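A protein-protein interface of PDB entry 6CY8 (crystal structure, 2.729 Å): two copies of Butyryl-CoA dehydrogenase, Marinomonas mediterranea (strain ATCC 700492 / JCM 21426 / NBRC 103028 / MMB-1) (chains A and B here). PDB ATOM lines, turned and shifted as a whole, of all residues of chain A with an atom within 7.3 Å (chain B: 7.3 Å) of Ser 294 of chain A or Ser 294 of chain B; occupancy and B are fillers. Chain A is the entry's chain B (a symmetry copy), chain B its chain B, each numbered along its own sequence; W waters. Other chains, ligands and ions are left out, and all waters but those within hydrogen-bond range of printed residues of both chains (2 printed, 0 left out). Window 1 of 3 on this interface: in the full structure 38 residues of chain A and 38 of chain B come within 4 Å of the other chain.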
ATOM      1  N   MET A 288      11.735   1.309   7.114  1.00  0.00           N
ATOM      2  CA  MET A 288      10.519   0.555   7.375  1.00  0.00           C
ATOM      3  C   MET A 288      10.842  -0.920   7.628  1.00  0.00           C
ATOM      4  O   MET A 288      10.304  -1.529   8.562  1.00  0.00           O
ATOM      5  CB  MET A 288       9.548   0.698   6.200  1.00  0.00           C
ATOM      6  CG  MET A 288       8.890   2.038   6.048  1.00  0.00           C
ATOM      7  SD  MET A 288       7.850   2.167   4.546  1.00  0.00           S
ATOM      8  CE  MET A 288       6.390   1.244   5.036  1.00  0.00           C
ATOM      9  N   GLY A 289      11.726  -1.507   6.816  1.00  0.00           N
ATOM     10  CA  GLY A 289      12.075  -2.904   7.007  1.00  0.00           C
ATOM     11  C   GLY A 289      12.886  -3.160   8.266  1.00  0.00           C
ATOM     12  O   GLY A 289      12.785  -4.230   8.873  1.00  0.00           O
ATOM     13  N   VAL A 290      13.719  -2.206   8.665  1.00  0.00           N
ATOM     14  CA  VAL A 290      14.496  -2.396   9.879  1.00  0.00           C
ATOM     15  C   VAL A 290      13.579  -2.377  11.094  1.00  0.00           C
ATOM     16  O   VAL A 290      13.591  -3.304  11.917  1.00  0.00           O
ATOM     17  CB  VAL A 290      15.594  -1.329   9.980  1.00  0.00           C
ATOM     18  CG1 VAL A 290      16.320  -1.457  11.310  1.00  0.00           C
ATOM     19  CG2 VAL A 290      16.535  -1.441   8.780  1.00  0.00           C
ATOM     20  N   ARG A 291      12.749  -1.330  11.212  1.00  0.00           N
ATOM     21  CA  ARG A 291      11.784  -1.266  12.307  1.00  0.00           C
ATOM     22  C   ARG A 291      10.849  -2.477  12.319  1.00  0.00           C
ATOM     23  O   ARG A 291      10.524  -2.995  13.396  1.00  0.00           O
ATOM     24  CB  ARG A 291      10.975   0.035  12.237  1.00  0.00           C
ATOM     25  CG  ARG A 291      11.811   1.265  12.360  1.00  0.00           C
ATOM     26  CD  ARG A 291      10.974   2.540  12.382  1.00  0.00           C
ATOM     27  NE  ARG A 291      10.051   2.679  11.256  1.00  0.00           N
ATOM     28  CZ  ARG A 291      10.268   3.448  10.194  1.00  0.00           C
ATOM     29  NH1 ARG A 291      11.395   4.134  10.077  1.00  0.00           N
ATOM     30  NH2 ARG A 291       9.359   3.513   9.239  1.00  0.00           N
ATOM     31  N   LEU A 292      10.403  -2.941  11.140  1.00  0.00           N
ATOM     32  CA  LEU A 292       9.553  -4.131  11.085  1.00  0.00           C
ATOM     33  C   LEU A 292      10.272  -5.356  11.644  1.00  0.00           C
ATOM     34  O   LEU A 292       9.723  -6.076  12.488  1.00  0.00           O
ATOM     35  CB  LEU A 292       9.090  -4.399   9.654  1.00  0.00           C
ATOM     36  CG  LEU A 292       7.750  -5.105   9.407  1.00  0.00           C
ATOM     37  CD1 LEU A 292       7.550  -5.350   7.909  1.00  0.00           C
ATOM     38  CD2 LEU A 292       7.604  -6.396  10.160  1.00  0.00           C
ATOM     39  N   GLU A 293      11.490  -5.629  11.169  1.00  0.00           N
ATOM     40  CA  GLU A 293      12.196  -6.805  11.665  1.00  0.00           C
ATOM     41  C   GLU A 293      12.470  -6.686  13.157  1.00  0.00           C
ATOM     42  O   GLU A 293      12.325  -7.659  13.904  1.00  0.00           O
ATOM     43  CB  GLU A 293      13.499  -7.018  10.905  1.00  0.00           C
ATOM     44  CG  GLU A 293      14.154  -8.358  11.233  1.00  0.00           C
ATOM     45  CD  GLU A 293      15.671  -8.342  11.071  1.00  0.00           C
ATOM     46  OE1 GLU A 293      16.377  -7.954  12.036  1.00  0.00           O
ATOM     47  OE2 GLU A 293      16.153  -8.724   9.977  1.00  0.00           O
ATOM     48  N   SER A 294      12.852  -5.494  13.606  1.00  0.00           N
ATOM     49  CA  SER A 294      12.962  -5.237  15.031  1.00  0.00           C
ATOM     50  C   SER A 294      11.652  -5.547  15.752  1.00  0.00           C
ATOM     51  O   SER A 294      11.638  -6.240  16.773  1.00  0.00           O
ATOM     52  CB  SER A 294      13.369  -3.780  15.253  1.00  0.00           C
ATOM     53  OG  SER A 294      13.135  -3.388  16.591  1.00  0.00           O
ATOM     54  N   ALA A 295      10.534  -5.038  15.227  1.00  0.00           N
ATOM     55  CA  ALA A 295       9.258  -5.184  15.925  1.00  0.00           C
ATOM     56  C   ALA A 295       8.804  -6.633  15.911  1.00  0.00           C
ATOM     57  O   ALA A 295       8.308  -7.148  16.920  1.00  0.00           O
ATOM     58  CB  ALA A 295       8.189  -4.292  15.287  1.00  0.00           C
ATOM     59  N   ARG A 296       8.950  -7.297  14.767  1.00  0.00           N
ATOM     60  CA  ARG A 296       8.596  -8.704  14.685  1.00  0.00           C
ATOM     61  C   ARG A 296       9.416  -9.532  15.664  1.00  0.00           C
ATOM     62  O   ARG A 296       8.872 -10.376  16.388  1.00  0.00           O
ATOM     63  CB  ARG A 296       8.782  -9.205  13.262  1.00  0.00           C
ATOM     64  CG  ARG A 296       8.510 -10.659  13.172  1.00  0.00           C
ATOM     65  CD  ARG A 296       8.644 -11.153  11.778  1.00  0.00           C
ATOM     66  NE  ARG A 296       7.652 -10.587  10.881  1.00  0.00           N
ATOM     67  CZ  ARG A 296       7.945  -9.821   9.836  1.00  0.00           C
ATOM     68  NH1 ARG A 296       9.205  -9.504   9.573  1.00  0.00           N
ATOM     69  NH2 ARG A 296       6.973  -9.373   9.052  1.00  0.00           N
ATOM     70  N   LEU A 297      10.729  -9.279  15.724  1.00  0.00           N
ATOM     71  CA  LEU A 297      11.588 -10.052  16.619  1.00  0.00           C
ATOM     72  C   LEU A 297      11.218  -9.825  18.083  1.00  0.00           C
ATOM     73  O   LEU A 297      11.181 -10.773  18.871  1.00  0.00           O
ATOM     74  CB  LEU A 297      13.056  -9.712  16.364  1.00  0.00           C
ATOM     75  CG  LEU A 297      13.631 -10.244  15.044  1.00  0.00           C
ATOM     76  CD1 LEU A 297      14.985  -9.593  14.695  1.00  0.00           C
ATOM     77  CD2 LEU A 297      13.732 -11.771  15.069  1.00  0.00           C
ATOM     78  N   MET A 298      10.931  -8.575  18.465  1.00  0.00           N
ATOM     79  CA  MET A 298      10.497  -8.284  19.829  1.00  0.00           C
ATOM     80  C   MET A 298       9.143  -8.906  20.130  1.00  0.00           C
ATOM     81  O   MET A 298       8.844  -9.249  21.287  1.00  0.00           O
ATOM     82  CB  MET A 298      10.422  -6.773  20.037  1.00  0.00           C
ATOM     83  CG  MET A 298      11.734  -6.104  19.791  1.00  0.00           C
ATOM     84  SD  MET A 298      11.603  -4.343  19.868  1.00  0.00           S
ATOM     85  CE  MET A 298      11.739  -4.160  21.644  1.00  0.00           C
ATOM     86  N   LEU A 299       8.299  -9.027  19.106  1.00  0.00           N
ATOM     87  CA  LEU A 299       7.028  -9.706  19.280  1.00  0.00           C
ATOM     88  C   LEU A 299       7.253 -11.178  19.598  1.00  0.00           C
ATOM     89  O   LEU A 299       6.768 -11.690  20.618  1.00  0.00           O
ATOM     90  CB  LEU A 299       6.183  -9.536  18.019  1.00  0.00           C
ATOM     91  CG  LEU A 299       4.952 -10.431  17.976  1.00  0.00           C
ATOM     92  CD1 LEU A 299       3.922  -9.979  19.022  1.00  0.00           C
ATOM     93  CD2 LEU A 299       4.374 -10.489  16.561  1.00  0.00           C
ATOM     94  N   TYR A 300       8.011 -11.866  18.739  1.00  0.00           N
ATOM     95  CA  TYR A 300       8.325 -13.272  18.962  1.00  0.00           C
ATOM     96  C   TYR A 300       8.974 -13.474  20.322  1.00  0.00           C
ATOM     97  O   TYR A 300       8.574 -14.361  21.088  1.00  0.00           O
ATOM     98  CB  TYR A 300       9.248 -13.780  17.854  1.00  0.00           C
ATOM     99  CG  TYR A 300       8.605 -13.830  16.500  1.00  0.00           C
ATOM    100  CD1 TYR A 300       7.225 -13.687  16.360  1.00  0.00           C
ATOM    101  CD2 TYR A 300       9.367 -14.040  15.358  1.00  0.00           C
ATOM    102  CE1 TYR A 300       6.622 -13.752  15.106  1.00  0.00           C
ATOM    103  CE2 TYR A 300       8.771 -14.104  14.098  1.00  0.00           C
ATOM    104  CZ  TYR A 300       7.401 -13.958  13.979  1.00  0.00           C
ATOM    105  OH  TYR A 300       6.828 -14.017  12.725  1.00  0.00           O
ATOM    106  N   MET A 318       7.755  -3.712  25.918  1.00  0.00           N
ATOM    107  CA  MET A 318       8.650  -3.301  24.848  1.00  0.00           C
ATOM    108  C   MET A 318       8.028  -3.609  23.488  1.00  0.00           C
ATOM    109  O   MET A 318       7.961  -2.739  22.614  1.00  0.00           O
ATOM    110  CB  MET A 318      10.011  -3.979  25.013  1.00  0.00           C
ATOM    111  CG  MET A 318      10.864  -3.386  26.122  1.00  0.00           C
ATOM    112  SD  MET A 318      12.593  -3.952  26.128  1.00  0.00           S
ATOM    113  CE  MET A 318      13.229  -3.093  27.606  1.00  0.00           C
ATOM    114  N   SER A 319       7.505  -4.823  23.323  1.00  0.00           N
ATOM    115  CA  SER A 319       6.939  -5.234  22.042  1.00  0.00           C
ATOM    116  C   SER A 319       5.766  -4.347  21.635  1.00  0.00           C
ATOM    117  O   SER A 319       5.659  -3.929  20.473  1.00  0.00           O
ATOM    118  CB  SER A 319       6.500  -6.694  22.125  1.00  0.00           C
ATOM    119  OG  SER A 319       5.911  -7.133  20.922  1.00  0.00           O
ATOM    120  N   ALA A 322       7.296  -0.869  20.648  1.00  0.00           N
ATOM    121  CA  ALA A 322       7.988  -0.950  19.372  1.00  0.00           C
ATOM    122  C   ALA A 322       7.018  -1.164  18.214  1.00  0.00           C
ATOM    123  O   ALA A 322       7.123  -0.499  17.172  1.00  0.00           O
ATOM    124  CB  ALA A 322       9.028  -2.070  19.433  1.00  0.00           C
ATOM    125  N   ILE A 323       6.062  -2.080  18.377  1.00  0.00           N
ATOM    126  CA  ILE A 323       5.152  -2.402  17.278  1.00  0.00           C
ATOM    127  C   ILE A 323       4.226  -1.225  16.981  1.00  0.00           C
ATOM    128  O   ILE A 323       4.036  -0.830  15.823  1.00  0.00           O
ATOM    129  CB  ILE A 323       4.359  -3.675  17.612  1.00  0.00           C
ATOM    130  CG1 ILE A 323       5.245  -4.895  17.483  1.00  0.00           C
ATOM    131  CG2 ILE A 323       3.130  -3.803  16.747  1.00  0.00           C
ATOM    132  CD1 ILE A 323       4.691  -6.097  18.233  1.00  0.00           C
ATOM    133  N   MET B 288      16.634   3.403  25.878  1.00  0.00           N
ATOM    134  CA  MET B 288      17.894   2.683  25.770  1.00  0.00           C
ATOM    135  C   MET B 288      17.659   1.172  25.827  1.00  0.00           C
ATOM    136  O   MET B 288      18.237   0.416  25.036  1.00  0.00           O
ATOM    137  CB  MET B 288      18.847   3.121  26.885  1.00  0.00           C
ATOM    138  CG  MET B 288      19.425   4.500  26.754  1.00  0.00           C
ATOM    139  SD  MET B 288      20.447   4.995  28.192  1.00  0.00           S
ATOM    140  CE  MET B 288      21.961   4.078  27.894  1.00  0.00           C
ATOM    141  N   GLY B 289      16.806   0.712  26.748  1.00  0.00           N
ATOM    142  CA  GLY B 289      16.541  -0.713  26.849  1.00  0.00           C
ATOM    143  C   GLY B 289      15.753  -1.268  25.676  1.00  0.00           C
ATOM    144  O   GLY B 289      15.921  -2.432  25.300  1.00  0.00           O
ATOM    145  N   VAL B 290      14.869  -0.466  25.094  1.00  0.00           N
ATOM    146  CA  VAL B 290      14.111  -0.946  23.950  1.00  0.00           C
ATOM    147  C   VAL B 290      15.034  -1.124  22.751  1.00  0.00           C
ATOM    148  O   VAL B 290      15.080  -2.199  22.135  1.00  0.00           O
ATOM    149  CB  VAL B 290      12.954   0.011  23.638  1.00  0.00           C
ATOM    150  CG1 VAL B 290      12.244  -0.431  22.367  1.00  0.00           C
ATOM    151  CG2 VAL B 290      12.013   0.093  24.841  1.00  0.00           C
ATOM    152  N   ARG B 291      15.801  -0.077  22.416  1.00  0.00           N
ATOM    153  CA  ARG B 291      16.767  -0.182  21.325  1.00  0.00           C
ATOM    154  C   ARG B 291      17.772  -1.313  21.556  1.00  0.00           C
ATOM    155  O   ARG B 291      18.133  -2.021  20.606  1.00  0.00           O
ATOM    156  CB  ARG B 291      17.498   1.150  21.121  1.00  0.00           C
ATOM    157  CG  ARG B 291      16.593   2.278  20.753  1.00  0.00           C
ATOM    158  CD  ARG B 291      17.353   3.568  20.466  1.00  0.00           C
ATOM    159  NE  ARG B 291      18.260   3.988  21.533  1.00  0.00           N
ATOM    160  CZ  ARG B 291      17.992   4.945  22.416  1.00  0.00           C
ATOM    161  NH1 ARG B 291      16.826   5.574  22.397  1.00  0.00           N
ATOM    162  NH2 ARG B 291      18.890   5.258  23.332  1.00  0.00           N
ATOM    163  N   LEU B 292      18.237  -1.498  22.802  1.00  0.00           N
ATOM    164  CA  LEU B 292      19.154  -2.599  23.096  1.00  0.00           C
ATOM    165  C   LEU B 292      18.512  -3.953  22.805  1.00  0.00           C
ATOM    166  O   LEU B 292      19.108  -4.798  22.122  1.00  0.00           O
ATOM    167  CB  LEU B 292      19.624  -2.541  24.548  1.00  0.00           C
ATOM    168  CG  LEU B 292      21.001  -3.102  24.927  1.00  0.00           C
ATOM    169  CD1 LEU B 292      21.206  -3.022  26.442  1.00  0.00           C
ATOM    170  CD2 LEU B 292      21.227  -4.508  24.454  1.00  0.00           C
ATOM    171  N   GLU B 293      17.309  -4.195  23.332  1.00  0.00           N
ATOM    172  CA  GLU B 293      16.676  -5.487  23.093  1.00  0.00           C
ATOM    173  C   GLU B 293      16.406  -5.692  21.609  1.00  0.00           C
ATOM    174  O   GLU B 293      16.611  -6.788  21.077  1.00  0.00           O
ATOM    175  CB  GLU B 293      15.384  -5.615  23.888  1.00  0.00           C
ATOM    176  CG  GLU B 293      14.810  -7.029  23.845  1.00  0.00           C
ATOM    177  CD  GLU B 293      13.294  -7.069  24.010  1.00  0.00           C
ATOM    178  OE1 GLU B 293      12.572  -6.929  22.991  1.00  0.00           O
ATOM    179  OE2 GLU B 293      12.828  -7.246  25.162  1.00  0.00           O
ATOM    180  N   SER B 294      15.957  -4.642  20.927  1.00  0.00           N
ATOM    181  CA  SER B 294      15.841  -4.690  19.481  1.00  0.00           C
ATOM    182  C   SER B 294      17.171  -5.064  18.831  1.00  0.00           C
ATOM    183  O   SER B 294      17.232  -5.949  17.974  1.00  0.00           O
ATOM    184  CB  SER B 294      15.350  -3.336  18.967  1.00  0.00           C
ATOM    185  OG  SER B 294      15.569  -3.213  17.576  1.00  0.00           O
ATOM    186  N   ALA B 295      18.254  -4.394  19.233  1.00  0.00           N
ATOM    187  CA  ALA B 295      19.540  -4.605  18.573  1.00  0.00           C
ATOM    188  C   ALA B 295      20.079  -5.990  18.881  1.00  0.00           C
ATOM    189  O   ALA B 295      20.609  -6.672  17.996  1.00  0.00           O
ATOM    190  CB  ALA B 295      20.551  -3.540  19.008  1.00  0.00           C
ATOM    191  N   ARG B 296      19.964  -6.413  20.138  1.00  0.00           N
ATOM    192  CA  ARG B 296      20.400  -7.750  20.505  1.00  0.00           C
ATOM    193  C   ARG B 296      19.635  -8.808  19.721  1.00  0.00           C
ATOM    194  O   ARG B 296      20.232  -9.750  19.183  1.00  0.00           O
ATOM    195  CB  ARG B 296      20.235  -7.959  22.001  1.00  0.00           C
ATOM    196  CG  ARG B 296      20.591  -9.345  22.386  1.00  0.00           C
ATOM    197  CD  ARG B 296      20.478  -9.549  23.852  1.00  0.00           C
ATOM    198  NE  ARG B 296      21.429  -8.754  24.608  1.00  0.00           N
ATOM    199  CZ  ARG B 296      21.085  -7.809  25.476  1.00  0.00           C
ATOM    200  NH1 ARG B 296      19.807  -7.519  25.676  1.00  0.00           N
ATOM    201  NH2 ARG B 296      22.025  -7.153  26.145  1.00  0.00           N
ATOM    202  N   LEU B 297      18.311  -8.650  19.619  1.00  0.00           N
ATOM    203  CA  LEU B 297      17.503  -9.640  18.906  1.00  0.00           C
ATOM    204  C   LEU B 297      17.869  -9.696  17.424  1.00  0.00           C
ATOM    205  O   LEU B 297      17.965 -10.782  16.847  1.00  0.00           O
ATOM    206  CB  LEU B 297      16.017  -9.342  19.095  1.00  0.00           C
ATOM    207  CG  LEU B 297      15.466  -9.623  20.500  1.00  0.00           C
ATOM    208  CD1 LEU B 297      14.074  -8.995  20.716  1.00  0.00           C
ATOM    209  CD2 LEU B 297      15.454 -11.127  20.790  1.00  0.00           C
ATOM    210  N   MET B 298      18.084  -8.536  16.793  1.00  0.00           N
ATOM    211  CA  MET B 298      18.508  -8.507  15.396  1.00  0.00           C
ATOM    212  C   MET B 298      19.898  -9.098  15.220  1.00  0.00           C
ATOM    213  O   MET B 298      20.224  -9.652  14.156  1.00  0.00           O
ATOM    214  CB  MET B 298      18.496  -7.070  14.882  1.00  0.00           C
ATOM    215  CG  MET B 298      17.146  -6.441  14.993  1.00  0.00           C
ATOM    216  SD  MET B 298      17.174  -4.730  14.556  1.00  0.00           S
ATOM    217  CE  MET B 298      17.038  -4.923  12.781  1.00  0.00           C
ATOM    218  N   LEU B 299      20.742  -8.956  16.242  1.00  0.00           N
ATOM    219  CA  LEU B 299      22.052  -9.581  16.204  1.00  0.00           C
ATOM    220  C   LEU B 299      21.915 -11.098  16.196  1.00  0.00           C
ATOM    221  O   LEU B 299      22.435 -11.777  15.300  1.00  0.00           O
ATOM    222  CB  LEU B 299      22.878  -9.106  17.397  1.00  0.00           C
ATOM    223  CG  LEU B 299      24.158  -9.901  17.615  1.00  0.00           C
ATOM    224  CD1 LEU B 299      25.167  -9.612  16.493  1.00  0.00           C
ATOM    225  CD2 LEU B 299      24.730  -9.632  19.009  1.00  0.00           C
ATOM    226  N   TYR B 300      21.194 -11.637  17.182  1.00  0.00           N
ATOM    227  CA  TYR B 300      20.963 -13.075  17.254  1.00  0.00           C
ATOM    228  C   TYR B 300      20.335 -13.590  15.969  1.00  0.00           C
ATOM    229  O   TYR B 300      20.791 -14.590  15.398  1.00  0.00           O
ATOM    230  CB  TYR B 300      20.065 -13.398  18.448  1.00  0.00           C
ATOM    231  CG  TYR B 300      20.702 -13.132  19.780  1.00  0.00           C
ATOM    232  CD1 TYR B 300      22.070 -12.883  19.880  1.00  0.00           C
ATOM    233  CD2 TYR B 300      19.946 -13.147  20.946  1.00  0.00           C
ATOM    234  CE1 TYR B 300      22.669 -12.652  21.117  1.00  0.00           C
ATOM    235  CE2 TYR B 300      20.537 -12.916  22.188  1.00  0.00           C
ATOM    236  CZ  TYR B 300      21.896 -12.669  22.267  1.00  0.00           C
ATOM    237  OH  TYR B 300      22.463 -12.434  23.502  1.00  0.00           O
ATOM    238  N   MET B 318      21.016  -5.130   8.481  1.00  0.00           N
ATOM    239  CA  MET B 318      20.092  -4.562   9.450  1.00  0.00           C
ATOM    240  C   MET B 318      20.722  -4.546  10.840  1.00  0.00           C
ATOM    241  O   MET B 318      20.733  -3.513  11.517  1.00  0.00           O
ATOM    242  CB  MET B 318      18.773  -5.336   9.435  1.00  0.00           C
ATOM    243  CG  MET B 318      17.894  -5.035   8.234  1.00  0.00           C
ATOM    244  SD  MET B 318      16.201  -5.690   8.354  1.00  0.00           S
ATOM    245  CE  MET B 318      15.525  -5.191   6.735  1.00  0.00           C
ATOM    246  N   SER B 319      21.315  -5.668  11.247  1.00  0.00           N
ATOM    247  CA  SER B 319      21.895  -5.773  12.582  1.00  0.00           C
ATOM    248  C   SER B 319      23.012  -4.754  12.791  1.00  0.00           C
ATOM    249  O   SER B 319      23.088  -4.101  13.842  1.00  0.00           O
ATOM    250  CB  SER B 319      22.419  -7.191  12.798  1.00  0.00           C
ATOM    251  OG  SER B 319      23.026  -7.338  14.062  1.00  0.00           O
ATOM    252  N   ALA B 322      21.275  -1.243  13.052  1.00  0.00           N
ATOM    253  CA  ALA B 322      20.581  -1.102  14.323  1.00  0.00           C
ATOM    254  C   ALA B 322      21.555  -1.016  15.494  1.00  0.00           C
ATOM    255  O   ALA B 322      21.405  -0.159  16.378  1.00  0.00           O
ATOM    256  CB  ALA B 322      19.609  -2.269  14.499  1.00  0.00           C
ATOM    257  N   ILE B 323      22.564  -1.888  15.517  1.00  0.00           N
ATOM    258  CA  ILE B 323      23.485  -1.925  16.653  1.00  0.00           C
ATOM    259  C   ILE B 323      24.339  -0.659  16.696  1.00  0.00           C
ATOM    260  O   ILE B 323      24.498  -0.025  17.747  1.00  0.00           O
ATOM    261  CB  ILE B 323      24.353  -3.190  16.583  1.00  0.00           C
ATOM    262  CG1 ILE B 323      23.539  -4.407  16.964  1.00  0.00           C
ATOM    263  CG2 ILE B 323      25.582  -3.066  17.448  1.00  0.00           C
ATOM    264  CD1 ILE B 323      24.167  -5.703  16.473  1.00  0.00           C
HETATM  265  O   HOH W   1      10.346  -8.018  23.408  1.00  0.00           O
HETATM  266  O   HOH W   2      18.665  -8.973  11.837  1.00  0.00           O
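The side-chain hydroxyl (OG) of Ser 294 of chain B lies within hydrogen-bond range of the side-chain hydroxyl (OG) of Ser 294 of chain A (2.6 Å).
The side-chain sulfur of Met 318 of chain B lies close to the backbone carbonyl oxygen of Gly 289 of chain A (3.8 Å).
The side-chain sulfur (SD) of Met 318 of chain B sits close to the side-chain carboxylate (OE2) of Glu 293 of chain A (3.4 Å).
The side-chain sulfur of Met 318 of chain A sits close to the backbone carbonyl oxygen of Gly 289 of chain B (3.8 Å).
The side-chain sulfur (SD) of Met 318 of chain A sits close to the side-chain carboxylate (OE2) of Glu 293 of chain B (3.4 Å).
SD of Met 298 of chain B lies within hydrogen-bond range of OG of Ser 294 of chain B, at 3.7 Å.
OG of Ser 294 of chain A sits at hydrogen-bond distance from SD of Met 298 of chain A, at 3.7 Å.
CG1 of Val 290 of chain A touches CE of Met 298 of chain B (3.8 Å).
Glu 293 of chain A touches Met 298 of chain B.
Met 298 of chain B touches Ser 294 of chain A.
O of Leu 297 of chain B touches CD1 of Leu 297 of chain A (3.9 Å).
Met 298 of chain B touches Leu 297 of chain A (CA to CD1, 3.8 Å).
CE of Met 298 of chain A touches CG1 of Val 290 of chain B, 3.8 Å away.
Glu 293 of chain B touches Met 298 of chain A.
Met 298 of chain A touches Ser 294 of chain B.
Met 298 of chain A touches Leu 297 of chain B.
Val 290 of chain B touches Met 318 of chain A (CG2 to CG, 3.9 Å).
Of the printed residues of chain B, Ser 294 of chain A touches Ser 294 and Met 298.
Of the printed residues of chain A, Ser 294 of chain B touches Ser 294 (2.6 Å) and Met 298 (3.98 Å).
Of the printed residues of chain A, Leu 297 of chain B touches Leu 297 (3.9 Å) and Met 298 (3.8 Å).
Of the printed residues of chain A, Glu 293 of chain B touches Met 298 and Met 318.
Of the printed residues of chain A, Met 298 of chain B touches Val 290, Glu 293, Ser 294 and Leu 297.
Leu 299 of chain B touches none of the printed residues of chain A.
The nearest printed residue of chain A that does not touch Ser 294 of chain B is Leu 297 of chain A (5.4 Å).
The nearest printed residue of chain A that does not touch Met 318 of chain B is Ser 294 of chain A (6.2 Å).
Printed residues of chain B that touch a printed residue of chain A: Gly 289, Val 290, Glu 293, Ser 294, Leu 297, Met 298 and Met 318.
Hydrophobic or aromatic side chains of chain B that line the printed part of chain A: Val 290, Leu 297, Met 298 and Met 318.
Along chain A the printed residues that touch a printed residue of chain B span positions 289 to 318.
Glu 293 of chain A touches Met 318 of chain B, and with the chains exchanged Met 318 of chain A touches Glu 293 of chain B.
Ser 294 of chain B touches its own counterpart, Ser 294 of chain A.
Leu 297 of chain A touches its own counterpart, Leu 297 of chain B.
Leu 297 of chain A touches Met 298 of chain B, and with the chains exchanged Met 298 of chain A touches Leu 297 of chain B.
17 positions are printed for both chains.
Of the 16 pairs that touch across the chains among the printed residues, 16 have their exchanged pair printed and touching as well.
Water W1 lies within hydrogen-bond range of the side-chain carboxylate of Glu 293 of chain B and the backbone carbonyl oxygen of Met 298 of chain A.
Water W2 bridges OE1 of Glu 293 of chain A and O of Met 298 of chain B.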
